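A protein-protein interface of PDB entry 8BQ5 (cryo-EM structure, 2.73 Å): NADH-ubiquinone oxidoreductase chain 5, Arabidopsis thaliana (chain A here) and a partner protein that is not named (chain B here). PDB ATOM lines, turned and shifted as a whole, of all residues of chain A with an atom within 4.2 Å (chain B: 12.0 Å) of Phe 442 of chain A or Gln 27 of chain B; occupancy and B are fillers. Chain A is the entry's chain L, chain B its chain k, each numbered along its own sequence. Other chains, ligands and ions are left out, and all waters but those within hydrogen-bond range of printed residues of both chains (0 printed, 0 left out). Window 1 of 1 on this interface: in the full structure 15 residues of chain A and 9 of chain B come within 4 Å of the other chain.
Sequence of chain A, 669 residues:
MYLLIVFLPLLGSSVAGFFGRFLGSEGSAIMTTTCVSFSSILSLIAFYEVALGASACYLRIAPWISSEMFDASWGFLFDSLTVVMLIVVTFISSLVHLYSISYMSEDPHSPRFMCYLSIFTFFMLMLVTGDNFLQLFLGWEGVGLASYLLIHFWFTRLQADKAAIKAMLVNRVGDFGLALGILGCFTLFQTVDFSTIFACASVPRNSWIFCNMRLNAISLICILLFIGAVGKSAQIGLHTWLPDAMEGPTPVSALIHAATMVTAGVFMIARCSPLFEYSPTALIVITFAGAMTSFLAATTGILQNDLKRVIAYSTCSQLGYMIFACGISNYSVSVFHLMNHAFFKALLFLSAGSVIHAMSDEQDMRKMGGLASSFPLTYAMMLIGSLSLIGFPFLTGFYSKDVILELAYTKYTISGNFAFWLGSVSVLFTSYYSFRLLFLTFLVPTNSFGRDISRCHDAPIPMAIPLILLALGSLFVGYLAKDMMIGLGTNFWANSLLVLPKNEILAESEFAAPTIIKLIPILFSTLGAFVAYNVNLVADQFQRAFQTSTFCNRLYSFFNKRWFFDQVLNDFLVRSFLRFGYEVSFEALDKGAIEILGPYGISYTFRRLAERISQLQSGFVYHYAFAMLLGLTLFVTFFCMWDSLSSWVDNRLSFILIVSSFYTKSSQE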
ATOM      1  N   GLY A 370       6.833   7.450  26.892  1.00  0.00           N
ATOM      2  CA  GLY A 370       7.373   8.656  27.558  1.00  0.00           C
ATOM      3  C   GLY A 370       8.499   9.229  26.718  1.00  0.00           C
ATOM      4  O   GLY A 370       8.659   8.728  25.620  1.00  0.00           O
ATOM      5  N   LEU A 371       9.241  10.234  27.199  1.00  0.00           N
ATOM      6  CA  LEU A 371      10.381  10.886  26.472  1.00  0.00           C
ATOM      7  C   LEU A 371       9.871  12.066  25.637  1.00  0.00           C
ATOM      8  O   LEU A 371      10.676  12.630  24.873  1.00  0.00           O
ATOM      9  CB  LEU A 371      11.193   9.911  25.601  1.00  0.00           C
ATOM     10  CG  LEU A 371      11.971   8.791  26.297  1.00  0.00           C
ATOM     11  CD1 LEU A 371      11.145   8.042  27.329  1.00  0.00           C
ATOM     12  CD2 LEU A 371      12.595   7.836  25.290  1.00  0.00           C
ATOM     13  N   ALA A 372       8.595  12.422  25.758  1.00  0.00           N
ATOM     14  CA  ALA A 372       8.109  13.647  25.078  1.00  0.00           C
ATOM     15  C   ALA A 372       8.723  14.854  25.783  1.00  0.00           C
ATOM     16  O   ALA A 372       8.915  15.887  25.121  1.00  0.00           O
ATOM     17  CB  ALA A 372       6.617  13.700  25.137  1.00  0.00           C
ATOM     18  N   SER A 373       9.007  14.723  27.082  1.00  0.00           N
ATOM     19  CA  SER A 373       9.645  15.810  27.862  1.00  0.00           C
ATOM     20  C   SER A 373      11.143  15.542  27.998  1.00  0.00           C
ATOM     21  O   SER A 373      11.908  16.517  28.008  1.00  0.00           O
ATOM     22  CB  SER A 373       9.017  15.904  29.216  1.00  0.00           C
ATOM     23  OG  SER A 373       7.604  15.815  29.128  1.00  0.00           O
ATOM     24  N   TYR A 379      12.130  14.927  19.950  1.00  0.00           N
ATOM     25  CA  TYR A 379      10.694  14.825  19.707  1.00  0.00           C
ATOM     26  C   TYR A 379      10.228  15.904  18.740  1.00  0.00           C
ATOM     27  O   TYR A 379       9.399  15.652  17.858  1.00  0.00           O
ATOM     28  CB  TYR A 379       9.919  14.935  21.017  1.00  0.00           C
ATOM     29  CG  TYR A 379       8.431  15.003  20.789  1.00  0.00           C
ATOM     30  CD1 TYR A 379       7.736  13.896  20.329  1.00  0.00           C
ATOM     31  CD2 TYR A 379       7.730  16.183  20.988  1.00  0.00           C
ATOM     32  CE1 TYR A 379       6.383  13.949  20.106  1.00  0.00           C
ATOM     33  CE2 TYR A 379       6.370  16.249  20.760  1.00  0.00           C
ATOM     34  CZ  TYR A 379       5.704  15.127  20.320  1.00  0.00           C
ATOM     35  OH  TYR A 379       4.350  15.174  20.091  1.00  0.00           O
ATOM     36  N   MET A 382      11.323  14.763  15.267  1.00  0.00           N
ATOM     37  CA  MET A 382      10.510  13.667  14.745  1.00  0.00           C
ATOM     38  C   MET A 382       9.093  14.131  14.449  1.00  0.00           C
ATOM     39  O   MET A 382       8.428  13.596  13.555  1.00  0.00           O
ATOM     40  CB  MET A 382      10.490  12.502  15.732  1.00  0.00           C
ATOM     41  CG  MET A 382      11.810  11.778  15.855  1.00  0.00           C
ATOM     42  SD  MET A 382      11.664   9.986  15.831  1.00  0.00           S
ATOM     43  CE  MET A 382      10.910   9.743  14.245  1.00  0.00           C
ATOM     44  N   LEU A 438       4.901   8.036  16.684  1.00  0.00           N
ATOM     45  CA  LEU A 438       4.916   9.215  17.547  1.00  0.00           C
ATOM     46  C   LEU A 438       4.306   8.908  18.907  1.00  0.00           C
ATOM     47  O   LEU A 438       4.826   9.328  19.947  1.00  0.00           O
ATOM     48  CB  LEU A 438       4.166  10.368  16.877  1.00  0.00           C
ATOM     49  CG  LEU A 438       5.031  11.432  16.211  1.00  0.00           C
ATOM     50  CD1 LEU A 438       6.015  12.005  17.208  1.00  0.00           C
ATOM     51  CD2 LEU A 438       5.768  10.824  15.048  1.00  0.00           C
ATOM     52  N   PHE A 439       3.196   8.173  18.917  1.00  0.00           N
ATOM     53  CA  PHE A 439       2.475   7.928  20.161  1.00  0.00           C
ATOM     54  C   PHE A 439       3.226   6.943  21.049  1.00  0.00           C
ATOM     55  O   PHE A 439       3.383   7.174  22.254  1.00  0.00           O
ATOM     56  CB  PHE A 439       1.074   7.414  19.839  1.00  0.00           C
ATOM     57  CG  PHE A 439       0.158   8.471  19.292  1.00  0.00           C
ATOM     58  CD1 PHE A 439       0.473   9.814  19.421  1.00  0.00           C
ATOM     59  CD2 PHE A 439      -0.992   8.122  18.608  1.00  0.00           C
ATOM     60  CE1 PHE A 439      -0.361  10.787  18.908  1.00  0.00           C
ATOM     61  CE2 PHE A 439      -1.825   9.090  18.089  1.00  0.00           C
ATOM     62  CZ  PHE A 439      -1.511  10.424  18.240  1.00  0.00           C
ATOM     63  N   LEU A 440       3.715   5.845  20.466  1.00  0.00           N
ATOM     64  CA  LEU A 440       4.316   4.782  21.267  1.00  0.00           C
ATOM     65  C   LEU A 440       5.703   5.163  21.769  1.00  0.00           C
ATOM     66  O   LEU A 440       6.166   4.631  22.784  1.00  0.00           O
ATOM     67  CB  LEU A 440       4.385   3.490  20.454  1.00  0.00           C
ATOM     68  CG  LEU A 440       3.063   2.768  20.194  1.00  0.00           C
ATOM     69  CD1 LEU A 440       3.294   1.511  19.373  1.00  0.00           C
ATOM     70  CD2 LEU A 440       2.371   2.436  21.504  1.00  0.00           C
ATOM     71  N   THR A 441       6.392   6.051  21.064  1.00  0.00           N
ATOM     72  CA  THR A 441       7.801   6.298  21.471  1.00  0.00           C
ATOM     73  C   THR A 441       7.872   7.423  22.503  1.00  0.00           C
ATOM     74  O   THR A 441       8.742   7.328  23.378  1.00  0.00           O
ATOM     75  CB  THR A 441       8.686   6.572  20.246  1.00  0.00           C
ATOM     76  OG1 THR A 441       8.539   5.478  19.340  1.00  0.00           O
ATOM     77  CG2 THR A 441      10.148   6.758  20.586  1.00  0.00           C
ATOM     78  N   PHE A 442       6.974   8.412  22.432  1.00  0.00           N
ATOM     79  CA  PHE A 442       7.126   9.592  23.322  1.00  0.00           C
ATOM     80  C   PHE A 442       5.872   9.999  24.089  1.00  0.00           C
ATOM     81  O   PHE A 442       6.040  10.657  25.119  1.00  0.00           O
ATOM     82  CB  PHE A 442       7.490  10.822  22.490  1.00  0.00           C
ATOM     83  CG  PHE A 442       8.566  10.648  21.448  1.00  0.00           C
ATOM     84  CD1 PHE A 442       9.902  10.797  21.778  1.00  0.00           C
ATOM     85  CD2 PHE A 442       8.238  10.390  20.126  1.00  0.00           C
ATOM     86  CE1 PHE A 442      10.889  10.656  20.817  1.00  0.00           C
ATOM     87  CE2 PHE A 442       9.226  10.250  19.165  1.00  0.00           C
ATOM     88  CZ  PHE A 442      10.549  10.383  19.513  1.00  0.00           C
ATOM     89  N   LEU A 443       4.679   9.588  23.674  1.00  0.00           N
ATOM     90  CA  LEU A 443       3.464  10.157  24.246  1.00  0.00           C
ATOM     91  C   LEU A 443       2.701   9.219  25.168  1.00  0.00           C
ATOM     92  O   LEU A 443       2.015   9.698  26.071  1.00  0.00           O
ATOM     93  CB  LEU A 443       2.537  10.632  23.121  1.00  0.00           C
ATOM     94  CG  LEU A 443       3.080  11.859  22.373  1.00  0.00           C
ATOM     95  CD1 LEU A 443       1.997  12.767  21.890  1.00  0.00           C
ATOM     96  CD2 LEU A 443       4.035  12.662  23.245  1.00  0.00           C
ATOM     97  N   VAL A 444       2.801   7.908  24.975  1.00  0.00           N
ATOM     98  CA  VAL A 444       2.126   6.946  25.845  1.00  0.00           C
ATOM     99  C   VAL A 444       2.818   6.913  27.203  1.00  0.00           C
ATOM    100  O   VAL A 444       3.959   7.381  27.325  1.00  0.00           O
ATOM    101  CB  VAL A 444       2.095   5.544  25.216  1.00  0.00           C
ATOM    102  CG1 VAL A 444       1.160   5.513  24.018  1.00  0.00           C
ATOM    103  CG2 VAL A 444       3.499   5.106  24.821  1.00  0.00           C
ATOM    104  N   TRP B  18       7.489   3.401  40.079  1.00  0.00           N
ATOM    105  CA  TRP B  18       8.377   4.453  39.598  1.00  0.00           C
ATOM    106  C   TRP B  18       7.874   5.099  38.317  1.00  0.00           C
ATOM    107  O   TRP B  18       8.296   6.213  37.989  1.00  0.00           O
ATOM    108  CB  TRP B  18       9.781   3.887  39.385  1.00  0.00           C
ATOM    109  CG  TRP B  18       9.873   2.875  38.275  1.00  0.00           C
ATOM    110  CD1 TRP B  18       9.756   1.522  38.394  1.00  0.00           C
ATOM    111  CD2 TRP B  18      10.126   3.134  36.887  1.00  0.00           C
ATOM    112  NE1 TRP B  18       9.907   0.923  37.169  1.00  0.00           N
ATOM    113  CE2 TRP B  18      10.136   1.890  36.227  1.00  0.00           C
ATOM    114  CE3 TRP B  18      10.338   4.295  36.139  1.00  0.00           C
ATOM    115  CZ2 TRP B  18      10.352   1.773  34.858  1.00  0.00           C
ATOM    116  CZ3 TRP B  18      10.552   4.177  34.780  1.00  0.00           C
ATOM    117  CH2 TRP B  18      10.558   2.926  34.153  1.00  0.00           C
ATOM    118  N   ARG B  19       6.975   4.432  37.592  1.00  0.00           N
ATOM    119  CA  ARG B  19       6.485   4.947  36.321  1.00  0.00           C
ATOM    120  C   ARG B  19       5.596   6.172  36.481  1.00  0.00           C
ATOM    121  O   ARG B  19       5.234   6.787  35.472  1.00  0.00           O
ATOM    122  CB  ARG B  19       5.732   3.848  35.575  1.00  0.00           C
ATOM    123  CG  ARG B  19       6.644   2.877  34.841  1.00  0.00           C
ATOM    124  CD  ARG B  19       5.903   1.618  34.443  1.00  0.00           C
ATOM    125  NE  ARG B  19       6.777   0.454  34.394  1.00  0.00           N
ATOM    126  CZ  ARG B  19       7.481   0.099  33.327  1.00  0.00           C
ATOM    127  NH1 ARG B  19       7.475   0.829  32.224  1.00  0.00           N
ATOM    128  NH2 ARG B  19       8.209  -1.012  33.369  1.00  0.00           N
ATOM    129  N   LYS B  20       5.225   6.532  37.710  1.00  0.00           N
ATOM    130  CA  LYS B  20       4.403   7.707  37.971  1.00  0.00           C
ATOM    131  C   LYS B  20       5.224   8.986  38.086  1.00  0.00           C
ATOM    132  O   LYS B  20       4.751   9.962  38.684  1.00  0.00           O
ATOM    133  CB  LYS B  20       3.577   7.497  39.243  1.00  0.00           C
ATOM    134  CG  LYS B  20       2.722   6.238  39.230  1.00  0.00           C
ATOM    135  CD  LYS B  20       1.959   6.095  37.921  1.00  0.00           C
ATOM    136  CE  LYS B  20       0.898   5.009  38.008  1.00  0.00           C
ATOM    137  NZ  LYS B  20      -0.409   5.468  37.456  1.00  0.00           N
ATOM    138  N   HIS B  21       6.426   8.991  37.521  1.00  0.00           N
ATOM    139  CA  HIS B  21       7.324  10.129  37.635  1.00  0.00           C
ATOM    140  C   HIS B  21       6.651  11.387  37.092  1.00  0.00           C
ATOM    141  O   HIS B  21       5.985  11.331  36.050  1.00  0.00           O
ATOM    142  CB  HIS B  21       8.617   9.851  36.864  1.00  0.00           C
ATOM    143  CG  HIS B  21       9.844  10.421  37.501  1.00  0.00           C
ATOM    144  ND1 HIS B  21      10.077  11.776  37.589  1.00  0.00           N
ATOM    145  CD2 HIS B  21      10.922   9.817  38.051  1.00  0.00           C
ATOM    146  CE1 HIS B  21      11.235  11.982  38.190  1.00  0.00           C
ATOM    147  NE2 HIS B  21      11.770  10.809  38.479  1.00  0.00           N
ATOM    148  N   PRO B  22       6.788  12.531  37.774  1.00  0.00           N
ATOM    149  CA  PRO B  22       6.160  13.765  37.271  1.00  0.00           C
ATOM    150  C   PRO B  22       6.488  14.079  35.823  1.00  0.00           C
ATOM    151  O   PRO B  22       5.579  14.392  35.045  1.00  0.00           O
ATOM    152  CB  PRO B  22       6.712  14.837  38.219  1.00  0.00           C
ATOM    153  CG  PRO B  22       6.968  14.107  39.485  1.00  0.00           C
ATOM    154  CD  PRO B  22       7.397  12.719  39.101  1.00  0.00           C
ATOM    155  N   MET B  23       7.756  13.984  35.429  1.00  0.00           N
ATOM    156  CA  MET B  23       8.157  14.267  34.059  1.00  0.00           C
ATOM    157  C   MET B  23       8.343  13.006  33.225  1.00  0.00           C
ATOM    158  O   MET B  23       9.005  13.055  32.184  1.00  0.00           O
ATOM    159  CB  MET B  23       9.429  15.115  34.037  1.00  0.00           C
ATOM    160  CG  MET B  23       9.227  16.513  34.611  1.00  0.00           C
ATOM    161  SD  MET B  23       7.981  17.445  33.692  1.00  0.00           S
ATOM    162  CE  MET B  23       8.790  17.664  32.109  1.00  0.00           C
ATOM    163  N   LEU B  24       7.671  11.917  33.619  1.00  0.00           N
ATOM    164  CA  LEU B  24       7.661  10.673  32.797  1.00  0.00           C
ATOM    165  C   LEU B  24       6.199  10.299  32.542  1.00  0.00           C
ATOM    166  O   LEU B  24       5.971   9.278  31.867  1.00  0.00           O
ATOM    167  CB  LEU B  24       8.379   9.544  33.537  1.00  0.00           C
ATOM    168  CG  LEU B  24       9.796   9.223  33.071  1.00  0.00           C
ATOM    169  CD1 LEU B  24      10.387   8.115  33.923  1.00  0.00           C
ATOM    170  CD2 LEU B  24       9.804   8.823  31.604  1.00  0.00           C
ATOM    171  N   SER B  25       5.247  11.067  33.084  1.00  0.00           N
ATOM    172  CA  SER B  25       3.830  10.859  32.834  1.00  0.00           C
ATOM    173  C   SER B  25       3.191  12.162  32.370  1.00  0.00           C
ATOM    174  O   SER B  25       3.796  13.236  32.435  1.00  0.00           O
ATOM    175  CB  SER B  25       3.118  10.334  34.088  1.00  0.00           C
ATOM    176  OG  SER B  25       3.409  11.144  35.213  1.00  0.00           O
ATOM    177  N   ASN B  26       1.916  12.065  31.963  1.00  0.00           N
ATOM    178  CA  ASN B  26       1.229  13.235  31.340  1.00  0.00           C
ATOM    179  C   ASN B  26       2.097  13.692  30.161  1.00  0.00           C
ATOM    180  O   ASN B  26       2.136  14.896  29.888  1.00  0.00           O
ATOM    181  CB  ASN B  26       0.859  14.354  32.323  1.00  0.00           C
ATOM    182  CG  ASN B  26       0.215  13.854  33.599  1.00  0.00           C
ATOM    183  OD1 ASN B  26      -0.650  12.982  33.568  1.00  0.00           O
ATOM    184  ND2 ASN B  26       0.628  14.406  34.728  1.00  0.00           N
ATOM    185  N   GLN B  27       2.736  12.739  29.471  1.00  0.00           N
ATOM    186  CA  GLN B  27       3.622  13.064  28.321  1.00  0.00           C
ATOM    187  C   GLN B  27       2.779  13.455  27.100  1.00  0.00           C
ATOM    188  O   GLN B  27       3.374  13.946  26.131  1.00  0.00           O
ATOM    189  CB  GLN B  27       4.550  11.879  28.043  1.00  0.00           C
ATOM    190  CG  GLN B  27       5.498  11.575  29.192  1.00  0.00           C
ATOM    191  CD  GLN B  27       6.459  12.711  29.435  1.00  0.00           C
ATOM    192  OE1 GLN B  27       7.285  13.040  28.588  1.00  0.00           O
ATOM    193  NE2 GLN B  27       6.358  13.319  30.605  1.00  0.00           N
ATOM    194  N   MET B  28       1.451  13.282  27.161  1.00  0.00           N
ATOM    195  CA  MET B  28       0.543  13.591  26.028  1.00  0.00           C
ATOM    196  C   MET B  28       0.119  15.064  26.059  1.00  0.00           C
ATOM    197  O   MET B  28      -0.610  15.471  25.135  1.00  0.00           O
ATOM    198  CB  MET B  28      -0.696  12.697  26.102  1.00  0.00           C
ATOM    199  CG  MET B  28      -1.647  12.894  24.940  1.00  0.00           C
ATOM    200  SD  MET B  28      -3.037  11.738  25.010  1.00  0.00           S
ATOM    201  CE  MET B  28      -2.250  10.249  24.400  1.00  0.00           C
ATOM    202  N   ARG B  29       0.521  15.822  27.082  1.00  0.00           N
ATOM    203  CA  ARG B  29       0.247  17.287  27.085  1.00  0.00           C
ATOM    204  C   ARG B  29       1.491  17.994  26.537  1.00  0.00           C
ATOM    205  O   ARG B  29       1.459  19.239  26.441  1.00  0.00           O
ATOM    206  CB  ARG B  29      -0.191  17.791  28.467  1.00  0.00           C
ATOM    207  CG  ARG B  29      -0.510  19.277  28.536  1.00  0.00           C
ATOM    208  CD  ARG B  29      -1.010  19.754  29.884  1.00  0.00           C
ATOM    209  NE  ARG B  29       0.017  19.619  30.907  1.00  0.00           N
ATOM    210  CZ  ARG B  29       0.988  20.496  31.126  1.00  0.00           C
ATOM    211  NH1 ARG B  29       1.072  21.594  30.395  1.00  0.00           N
ATOM    212  NH2 ARG B  29       1.873  20.273  32.082  1.00  0.00           N
ATOM    213  N   HIS B  30       2.538  17.239  26.188  1.00  0.00           N
ATOM    214  CA  HIS B  30       3.740  17.825  25.530  1.00  0.00           C
ATOM    215  C   HIS B  30       3.663  17.526  24.036  1.00  0.00           C
ATOM    216  O   HIS B  30       4.683  17.719  23.352  1.00  0.00           O
ATOM    217  CB  HIS B  30       5.018  17.268  26.155  1.00  0.00           C
ATOM    218  CG  HIS B  30       5.077  17.433  27.635  1.00  0.00           C
ATOM    219  ND1 HIS B  30       4.525  16.514  28.505  1.00  0.00           N
ATOM    220  CD2 HIS B  30       5.618  18.404  28.402  1.00  0.00           C
ATOM    221  CE1 HIS B  30       4.717  16.915  29.744  1.00  0.00           C
ATOM    222  NE2 HIS B  30       5.390  18.069  29.707  1.00  0.00           N
ATOM    223  N   ALA B  31       2.494  17.088  23.555  1.00  0.00           N
ATOM    224  CA  ALA B  31       2.324  16.688  22.139  1.00  0.00           C
ATOM    225  C   ALA B  31       2.636  17.829  21.169  1.00  0.00           C
ATOM    226  O   ALA B  31       3.071  17.515  20.060  1.00  0.00           O
ATOM    227  CB  ALA B  31       0.912  16.192  21.934  1.00  0.00           C
ATOM    228  N   LEU B  32       2.429  19.093  21.550  1.00  0.00           N
ATOM    229  CA  LEU B  32       2.585  20.195  20.604  1.00  0.00           C
ATOM    230  C   LEU B  32       3.468  21.279  21.214  1.00  0.00           C
ATOM    231  O   LEU B  32       2.969  22.268  21.766  1.00  0.00           O
ATOM    232  CB  LEU B  32       1.232  20.769  20.191  1.00  0.00           C
ATOM    233  CG  LEU B  32       0.233  19.765  19.611  1.00  0.00           C
ATOM    234  CD1 LEU B  32      -1.131  20.409  19.427  1.00  0.00           C
ATOM    235  CD2 LEU B  32       0.740  19.186  18.301  1.00  0.00           C
ATOM    236  N   PRO B  33       4.787  21.118  21.137  1.00  0.00           N
ATOM    237  CA  PRO B  33       5.683  22.192  21.578  1.00  0.00           C
ATOM    238  C   PRO B  33       5.478  23.453  20.754  1.00  0.00           C
ATOM    239  O   PRO B  33       5.206  23.396  19.552  1.00  0.00           O
ATOM    240  CB  PRO B  33       7.083  21.608  21.357  1.00  0.00           C
ATOM    241  CG  PRO B  33       6.892  20.478  20.400  1.00  0.00           C
ATOM    242  CD  PRO B  33       5.520  19.943  20.642  1.00  0.00           C
ATOM    243  N   GLY B  34       5.601  24.600  21.419  1.00  0.00           N
ATOM    244  CA  GLY B  34       5.523  25.881  20.746  1.00  0.00           C
ATOM    245  C   GLY B  34       4.191  26.215  20.116  1.00  0.00           C
ATOM    246  O   GLY B  34       4.133  27.127  19.285  1.00  0.00           O
ATOM    247  N   ILE B  35       3.116  25.507  20.470  1.00  0.00           N
ATOM    248  CA  ILE B  35       1.811  25.825  19.897  1.00  0.00           C
ATOM    249  C   ILE B  35       1.303  27.166  20.417  1.00  0.00           C
ATOM    250  O   ILE B  35       0.729  27.955  19.657  1.00  0.00           O
ATOM    251  CB  ILE B  35       0.812  24.680  20.164  1.00  0.00           C
ATOM    252  CG1 ILE B  35      -0.518  24.930  19.441  1.00  0.00           C
ATOM    253  CG2 ILE B  35       0.598  24.461  21.657  1.00  0.00           C
ATOM    254  CD1 ILE B  35      -0.475  24.681  17.946  1.00  0.00           C
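OE1 of Gln 27 of chain B is in hydrogen-bond range of N of Ala 372 of chain A (3.2 Å).
The backbone NH of Ser 373 of chain A sits at hydrogen-bond distance from the side-chain amide oxygen of Gln 27 of chain B (2.8 Å).
The side-chain hydroxyl (OG) of Ser 373 of chain A sits close to a ring nitrogen (NE2) of His 30 of chain B.
The backbone carbonyl oxygen (O) of Ala 31 of chain B is in hydrogen-bond range of the side-chain hydroxyl (OH) of Tyr 379 of chain A, at 2.7 Å.
O of Gly 370 of chain A sits close to O of Thr 441 of chain A, 2.6 Å away.
The backbone carbonyl oxygen (O) of Val 444 of chain A is in hydrogen-bond range of the backbone NH (N) of Gly 370 of chain A (2.9 Å).
The backbone NH of Ala 372 of chain A sits close to the backbone carbonyl oxygen of Phe 442 of chain A (3.2 Å).
O of Met 23 of chain B is in hydrogen-bond range of NE2 of Gln 27 of chain B (3.1 Å).
O of Ser 25 of chain B lies within hydrogen-bond range of NE2 of Gln 27 of chain B (3.1 Å).
A ring nitrogen (ND1) of His 30 of chain B lies within hydrogen-bond range of the backbone carbonyl oxygen (O) of Asn 26 of chain B.
Gln 27 of chain B touches Gly 370 of chain A (CG to CA, 3.8 Å).
Leu 371 of chain A touches Gln 27 of chain B.
Met 23 of chain B touches Ser 373 of chain A.
Tyr 379 of chain A touches His 30 of chain B (CE2 to O, 3.4 Å).
CD of Pro 33 of chain B touches CE2 of Tyr 379 of chain A, at 3.8 Å.
Phe 442 of chain A touches Gln 27 of chain B (O to CB, 3.5 Å).
Gln 27 of chain B touches Leu 443 of chain A (O to CD2, 3.2 Å).
O of Leu 443 of chain A touches N of Met 28 of chain B (3.8 Å).
CB of Ala 31 of chain B touches CD1 of Leu 443 of chain A, at 3.6 Å.
Phe 442 of chain A touches just one residue of chain B: Gln 27 (3.5 Å).
Of chain A, only Gly 370 (3.8 Å), Leu 371 (3.7 Å), Ala 372 (3.2 Å), Ser 373 (2.8 Å), Phe 442 (3.5 Å) and Leu 443 (3.2 Å) come within 4 Å of Gln 27 of chain B.
Gly 370 of chain A touches just one residue of chain B: Gln 27 (3.8 Å).
Printed residues of chain B within 4 Å of Ala 372 of chain A: Gln 27.
Of chain B, only Met 23 (3.4 Å), Gln 27 (2.8 Å) and His 30 (3.2 Å) come within 4 Å of Ser 373 of chain A.
Tyr 379 of chain A touches just these residues of chain B: His 30 (3.4 Å), Ala 31 (2.7 Å) and Pro 33 (3.8 Å).
No residue of chain B comes within 4 Å of Met 382 of chain A.
No residue of chain B comes within 4 Å of Thr 441 of chain A.
No residue of chain B comes within 4 Å of Val 444 of chain A.
Printed residues of chain A within 4 Å of Met 28 of chain B: Leu 443 (3.8 Å).
Of the printed residues of chain A, Pro 33 of chain B touches Tyr 379.
Of the printed residues of chain A, Ala 31 of chain B touches Tyr 379 and Leu 443.
Printed residues of chain A within 4 Å of Met 23 of chain B: Ser 373 (3.4 Å).
Arg 29 of chain B touches none of the printed residues of chain A.
The nearest printed residue of chain A that does not touch Gln 27 of chain B is Val 444 of chain A (4.6 Å).
Hydrophobic or aromatic side chains of chain A that line the printed part of chain B: Ala 372, Tyr 379 and Leu 443.
Of the 18 printed residues of chain B, 6 touch a printed residue of chain A.
Hydrophobic or aromatic side chains of chain B within 4 Å of the printed part of chain A: Met 23, His 30, Ala 31 and Pro 33.
Among the printed residues, no Asp or Glu carboxylate lies within 4 Å of a Lys or Arg side-chain nitrogen of the other chain.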
